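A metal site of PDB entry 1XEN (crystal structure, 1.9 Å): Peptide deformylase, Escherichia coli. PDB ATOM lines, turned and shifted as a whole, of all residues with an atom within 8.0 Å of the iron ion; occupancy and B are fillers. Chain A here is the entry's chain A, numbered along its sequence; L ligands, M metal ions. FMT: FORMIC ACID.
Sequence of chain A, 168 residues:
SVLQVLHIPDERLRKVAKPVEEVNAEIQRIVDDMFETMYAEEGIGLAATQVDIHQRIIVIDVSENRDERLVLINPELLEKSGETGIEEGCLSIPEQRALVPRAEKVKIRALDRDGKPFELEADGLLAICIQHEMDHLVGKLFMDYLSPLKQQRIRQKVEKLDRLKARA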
ATOM      1  N   VAL A   5      27.599   8.882 -19.100  1.00  0.00           N
ATOM      2  CA  VAL A   5      26.257   8.614 -19.631  1.00  0.00           C
ATOM      3  C   VAL A   5      26.164   9.139 -21.056  1.00  0.00           C
ATOM      4  O   VAL A   5      26.443  10.324 -21.310  1.00  0.00           O
ATOM      5  CB  VAL A   5      25.194   9.310 -18.755  1.00  0.00           C
ATOM      6  CG1 VAL A   5      23.798   9.109 -19.377  1.00  0.00           C
ATOM      7  CG2 VAL A   5      25.256   8.749 -17.313  1.00  0.00           C
ATOM      8  N   LEU A  13      22.684   4.260 -28.017  1.00  0.00           N
ATOM      9  CA  LEU A  13      21.462   4.298 -27.203  1.00  0.00           C
ATOM     10  C   LEU A  13      20.324   3.470 -27.841  1.00  0.00           C
ATOM     11  O   LEU A  13      19.305   3.232 -27.169  1.00  0.00           O
ATOM     12  CB  LEU A  13      20.981   5.754 -26.983  1.00  0.00           C
ATOM     13  CG  LEU A  13      21.859   6.523 -25.986  1.00  0.00           C
ATOM     14  CD1 LEU A  13      21.538   8.043 -26.049  1.00  0.00           C
ATOM     15  CD2 LEU A  13      21.608   5.956 -24.560  1.00  0.00           C
ATOM     16  N   GLY A  45      16.634   6.632 -12.087  1.00  0.00           N
ATOM     17  CA  GLY A  45      16.775   5.334 -12.752  1.00  0.00           C
ATOM     18  C   GLY A  45      17.928   5.400 -13.763  1.00  0.00           C
ATOM     19  O   GLY A  45      18.312   6.466 -14.227  1.00  0.00           O
ATOM     20  N   LEU A  46      18.491   4.261 -14.099  1.00  0.00           N
ATOM     21  CA  LEU A  46      19.563   4.261 -15.103  1.00  0.00           C
ATOM     22  C   LEU A  46      19.584   2.877 -15.730  1.00  0.00           C
ATOM     23  O   LEU A  46      19.531   1.888 -15.000  1.00  0.00           O
ATOM     24  CB  LEU A  46      20.931   4.566 -14.434  1.00  0.00           C
ATOM     25  CG  LEU A  46      22.135   4.596 -15.399  1.00  0.00           C
ATOM     26  CD1 LEU A  46      22.039   5.875 -16.372  1.00  0.00           C
ATOM     27  CD2 LEU A  46      23.439   4.664 -14.594  1.00  0.00           C
ATOM     28  N   ALA A  47      19.601   2.792 -17.065  1.00  0.00           N
ATOM     29  CA  ALA A  47      19.696   1.504 -17.754  1.00  0.00           C
ATOM     30  C   ALA A  47      21.147   1.304 -18.216  1.00  0.00           C
ATOM     31  O   ALA A  47      21.807   2.258 -18.617  1.00  0.00           O
ATOM     32  CB  ALA A  47      18.759   1.470 -18.929  1.00  0.00           C
ATOM     33  N   GLN A  50      22.569   3.052 -21.345  1.00  0.00           N
ATOM     34  CA  GLN A  50      22.952   4.472 -21.226  1.00  0.00           C
ATOM     35  C   GLN A  50      24.408   4.691 -20.861  1.00  0.00           C
ATOM     36  O   GLN A  50      24.901   5.796 -21.048  1.00  0.00           O
ATOM     37  CB  GLN A  50      22.100   5.211 -20.183  1.00  0.00           C
ATOM     38  CG  GLN A  50      20.634   5.196 -20.506  1.00  0.00           C
ATOM     39  CD  GLN A  50      19.846   5.926 -19.457  1.00  0.00           C
ATOM     40  OE1 GLN A  50      19.366   5.326 -18.487  1.00  0.00           O
ATOM     41  NE2 GLN A  50      19.744   7.255 -19.611  1.00  0.00           N
ATOM     42  N   GLU A  88       8.340  13.434 -18.328  1.00  0.00           N
ATOM     43  CA  GLU A  88       9.558  12.702 -18.032  1.00  0.00           C
ATOM     44  C   GLU A  88      10.778  13.389 -18.544  1.00  0.00           C
ATOM     45  O   GLU A  88      10.732  14.004 -19.604  1.00  0.00           O
ATOM     46  CB  GLU A  88       9.507  11.338 -18.749  1.00  0.00           C
ATOM     47  CG  GLU A  88       8.299  10.453 -18.291  1.00  0.00           C
ATOM     48  CD  GLU A  88       8.312   9.019 -18.877  1.00  0.00           C
ATOM     49  OE1 GLU A  88       9.392   8.592 -19.345  1.00  0.00           O
ATOM     50  OE2 GLU A  88       7.252   8.316 -18.849  1.00  0.00           O
ATOM     51  N   GLY A  89      11.877  13.172 -17.824  1.00  0.00           N
ATOM     52  CA  GLY A  89      13.177  13.632 -18.275  1.00  0.00           C
ATOM     53  C   GLY A  89      14.005  12.367 -18.509  1.00  0.00           C
ATOM     54  O   GLY A  89      13.514  11.248 -18.311  1.00  0.00           O
ATOM     55  N   CYS A  90      15.267  12.543 -18.866  1.00  0.00           N
ATOM     56  CA  CYS A  90      16.144  11.397 -19.120  1.00  0.00           C
ATOM     57  C   CYS A  90      17.557  11.861 -19.041  1.00  0.00           C
ATOM     58  O   CYS A  90      17.888  12.922 -19.591  1.00  0.00           O
ATOM     59  CB  CYS A  90      15.880  10.843 -20.534  1.00  0.00           C
ATOM     60  SG  CYS A  90      16.874   9.408 -21.012  1.00  0.00           S
ATOM     61  N   LEU A  91      18.416  11.088 -18.367  1.00  0.00           N
ATOM     62  CA  LEU A  91      19.822  11.484 -18.269  1.00  0.00           C
ATOM     63  C   LEU A  91      20.503  11.541 -19.621  1.00  0.00           C
ATOM     64  O   LEU A  91      21.534  12.216 -19.776  1.00  0.00           O
ATOM     65  CB  LEU A  91      20.587  10.506 -17.361  1.00  0.00           C
ATOM     66  CG  LEU A  91      20.014  10.448 -15.957  1.00  0.00           C
ATOM     67  CD1 LEU A  91      20.839   9.405 -15.136  1.00  0.00           C
ATOM     68  CD2 LEU A  91      20.085  11.818 -15.271  1.00  0.00           C
ATOM     69  N   SER A  92      19.954  10.840 -20.614  1.00  0.00           N
ATOM     70  CA  SER A  92      20.558  10.832 -21.949  1.00  0.00           C
ATOM     71  C   SER A  92      19.955  11.915 -22.859  1.00  0.00           C
ATOM     72  O   SER A  92      20.356  12.043 -24.019  1.00  0.00           O
ATOM     73  CB  SER A  92      20.382   9.473 -22.612  1.00  0.00           C
ATOM     74  OG  SER A  92      21.106   8.445 -21.945  1.00  0.00           O
ATOM     75  N   ILE A  93      19.008  12.693 -22.325  1.00  0.00           N
ATOM     76  CA  ILE A  93      18.375  13.779 -23.103  1.00  0.00           C
ATOM     77  C   ILE A  93      18.328  14.966 -22.120  1.00  0.00           C
ATOM     78  O   ILE A  93      17.289  15.448 -21.729  1.00  0.00           O
ATOM     79  CB  ILE A  93      16.951  13.373 -23.575  1.00  0.00           C
ATOM     80  CG1 ILE A  93      17.004  11.971 -24.247  1.00  0.00           C
ATOM     81  CG2 ILE A  93      16.412  14.415 -24.553  1.00  0.00           C
ATOM     82  CD1 ILE A  93      15.632  11.468 -24.789  1.00  0.00           C
ATOM     83  N   ARG A 102       1.947   6.138 -20.436  1.00  0.00           N
ATOM     84  CA  ARG A 102       2.492   4.951 -19.798  1.00  0.00           C
ATOM     85  C   ARG A 102       1.354   4.180 -19.139  1.00  0.00           C
ATOM     86  O   ARG A 102       0.282   4.722 -18.859  1.00  0.00           O
ATOM     87  CB  ARG A 102       3.464   5.356 -18.669  1.00  0.00           C
ATOM     88  CG  ARG A 102       4.720   6.140 -19.128  1.00  0.00           C
ATOM     89  CD  ARG A 102       5.733   5.223 -19.844  1.00  0.00           C
ATOM     90  NE  ARG A 102       6.983   5.928 -20.108  1.00  0.00           N
ATOM     91  CZ  ARG A 102       7.959   5.457 -20.877  1.00  0.00           C
ATOM     92  NH1 ARG A 102       7.815   4.249 -21.468  1.00  0.00           N
ATOM     93  NH2 ARG A 102       9.074   6.184 -21.085  1.00  0.00           N
ATOM     94  N   CYS A 129       8.772   4.920 -13.955  1.00  0.00           N
ATOM     95  CA  CYS A 129      10.239   4.793 -14.004  1.00  0.00           C
ATOM     96  C   CYS A 129      10.637   3.408 -14.554  1.00  0.00           C
ATOM     97  O   CYS A 129      11.498   3.267 -15.410  1.00  0.00           O
ATOM     98  CB  CYS A 129      10.822   4.983 -12.578  1.00  0.00           C
ATOM     99  SG  CYS A 129      12.603   4.823 -12.532  1.00  0.00           S
ATOM    100  N   HIS A 132      10.136   3.332 -18.290  1.00  0.00           N
ATOM    101  CA  HIS A 132      11.138   4.187 -18.962  1.00  0.00           C
ATOM    102  C   HIS A 132      12.480   3.431 -18.992  1.00  0.00           C
ATOM    103  O   HIS A 132      13.176   3.406 -20.059  1.00  0.00           O
ATOM    104  CB  HIS A 132      11.220   5.507 -18.167  1.00  0.00           C
ATOM    105  CG  HIS A 132      12.277   6.433 -18.651  1.00  0.00           C
ATOM    106  ND1 HIS A 132      12.041   7.677 -19.176  1.00  0.00           N
ATOM    107  CD2 HIS A 132      13.635   6.291 -18.618  1.00  0.00           C
ATOM    108  CE1 HIS A 132      13.232   8.250 -19.459  1.00  0.00           C
ATOM    109  NE2 HIS A 132      14.236   7.456 -19.119  1.00  0.00           N
ATOM    110  N   GLU A 133      12.881   2.816 -17.868  1.00  0.00           N
ATOM    111  CA  GLU A 133      14.170   2.088 -17.910  1.00  0.00           C
ATOM    112  C   GLU A 133      14.131   0.840 -18.806  1.00  0.00           C
ATOM    113  O   GLU A 133      15.113   0.552 -19.506  1.00  0.00           O
ATOM    114  CB  GLU A 133      14.698   1.727 -16.502  1.00  0.00           C
ATOM    115  CG  GLU A 133      14.700   2.854 -15.481  1.00  0.00           C
ATOM    116  CD  GLU A 133      15.418   4.095 -15.984  1.00  0.00           C
ATOM    117  OE1 GLU A 133      16.372   3.968 -16.795  1.00  0.00           O
ATOM    118  OE2 GLU A 133      15.009   5.196 -15.559  1.00  0.00           O
ATOM    119  N   ASP A 135      12.353   0.473 -21.414  1.00  0.00           N
ATOM    120  CA  ASP A 135      12.413   0.935 -22.814  1.00  0.00           C
ATOM    121  C   ASP A 135      13.893   1.120 -23.234  1.00  0.00           C
ATOM    122  O   ASP A 135      14.271   0.766 -24.354  1.00  0.00           O
ATOM    123  CB  ASP A 135      11.688   2.290 -22.994  1.00  0.00           C
ATOM    124  CG  ASP A 135      10.216   2.155 -23.347  1.00  0.00           C
ATOM    125  OD1 ASP A 135       9.710   1.002 -23.446  1.00  0.00           O
ATOM    126  OD2 ASP A 135       9.545   3.228 -23.516  1.00  0.00           O
ATOM    127  N   HIS A 136      14.743   1.661 -22.336  1.00  0.00           N
ATOM    128  CA  HIS A 136      16.140   1.879 -22.712  1.00  0.00           C
ATOM    129  C   HIS A 136      16.825   0.607 -23.134  1.00  0.00           C
ATOM    130  O   HIS A 136      17.698   0.643 -23.999  1.00  0.00           O
ATOM    131  CB  HIS A 136      16.987   2.401 -21.549  1.00  0.00           C
ATOM    132  CG  HIS A 136      16.920   3.878 -21.359  1.00  0.00           C
ATOM    133  ND1 HIS A 136      17.305   4.781 -22.335  1.00  0.00           N
ATOM    134  CD2 HIS A 136      16.566   4.601 -20.258  1.00  0.00           C
ATOM    135  CE1 HIS A 136      17.178   6.016 -21.791  1.00  0.00           C
ATOM    136  NE2 HIS A 136      16.737   5.955 -20.555  1.00  0.00           N
ATOM    137  N   LYS A 140      14.842   2.151 -26.851  1.00  0.00           N
ATOM    138  CA  LYS A 140      13.709   3.084 -27.026  1.00  0.00           C
ATOM    139  C   LYS A 140      13.872   4.221 -26.021  1.00  0.00           C
ATOM    140  O   LYS A 140      14.276   3.972 -24.853  1.00  0.00           O
ATOM    141  CB  LYS A 140      12.399   2.314 -26.817  1.00  0.00           C
ATOM    142  CG  LYS A 140      11.080   3.108 -26.900  1.00  0.00           C
ATOM    143  CD  LYS A 140       9.894   2.119 -26.825  1.00  0.00           C
ATOM    144  CE  LYS A 140       8.584   2.669 -27.416  1.00  0.00           C
ATOM    145  NZ  LYS A 140       7.423   1.728 -27.192  1.00  0.00           N
ATOM    146  N   LEU A 141      13.598   5.461 -26.465  1.00  0.00           N
ATOM    147  CA  LEU A 141      13.746   6.643 -25.610  1.00  0.00           C
ATOM    148  C   LEU A 141      12.407   7.319 -25.477  1.00  0.00           C
ATOM    149  O   LEU A 141      11.531   7.155 -26.350  1.00  0.00           O
ATOM    150  CB  LEU A 141      14.745   7.629 -26.226  1.00  0.00           C
ATOM    151  CG  LEU A 141      16.137   7.074 -26.557  1.00  0.00           C
ATOM    152  CD1 LEU A 141      16.919   8.105 -27.433  1.00  0.00           C
ATOM    153  CD2 LEU A 141      16.901   6.787 -25.236  1.00  0.00           C
ATOM    154  N   PHE A 142      12.241   8.114 -24.431  1.00  0.00           N
ATOM    155  CA  PHE A 142      10.891   8.668 -24.261  1.00  0.00           C
ATOM    156  C   PHE A 142      10.481   9.594 -25.395  1.00  0.00           C
ATOM    157  O   PHE A 142       9.295   9.748 -25.657  1.00  0.00           O
ATOM    158  CB  PHE A 142      10.748   9.378 -22.890  1.00  0.00           C
ATOM    159  CG  PHE A 142      11.292  10.798 -22.852  1.00  0.00           C
ATOM    160  CD1 PHE A 142      10.545  11.872 -23.338  1.00  0.00           C
ATOM    161  CD2 PHE A 142      12.527  11.060 -22.274  1.00  0.00           C
ATOM    162  CE1 PHE A 142      11.035  13.208 -23.236  1.00  0.00           C
ATOM    163  CE2 PHE A 142      13.027  12.388 -22.165  1.00  0.00           C
ATOM    164  CZ  PHE A 142      12.281  13.449 -22.640  1.00  0.00           C
HETATM  165  C   FMT L   1      16.894   7.545 -16.806  1.00  0.00           C
HETATM  166  O1  FMT L   1      16.751   6.267 -17.524  1.00  0.00           O
HETATM  167  O2  FMT L   1      17.611   8.516 -17.714  1.00  0.00           O
HETATM  168 FE    FE M   1      16.311   7.717 -19.444  1.00  0.00          FE
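A ring nitrogen (ND1) of His 132 is in hydrogen-bond range of the side-chain carboxylate of Glu 88 (2.8 Å).
The side-chain amide oxygen of Gln 50 sits at hydrogen-bond distance from the backbone NH of Ala 47 (2.9 Å).
The side-chain amide oxygen (OE1) of Gln 50 lies close to a ring nitrogen (NE2) of His 136 (3.4 Å).
The side-chain amide nitrogen (NE2) of Gln 50 sits at hydrogen-bond distance from the side-chain hydroxyl (OG) of Ser 92, 3.0 Å away.
N of Ser 92 sits close to SG of Cys 90, 3.4 Å away.
Residues that only touch the iron ion: Gln 50.
Within 4 Å of the iron ion: Gln 50, Cys 90, His 132 and His 136.
The nearest printed residue that does not touch the iron ion is Leu 91 (4.1 Å).
The iron ion is bound by a ring nitrogen (NE2) of His 132 (2.1 Å), a ring nitrogen (NE2) of His 136 (2.1 Å), an oxygen (O2) of the ligand (2.3 Å), the side-chain sulfur (SG) of Cys 90 (2.4 Å) and an oxygen (O1) of the ligand (2.4 Å).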
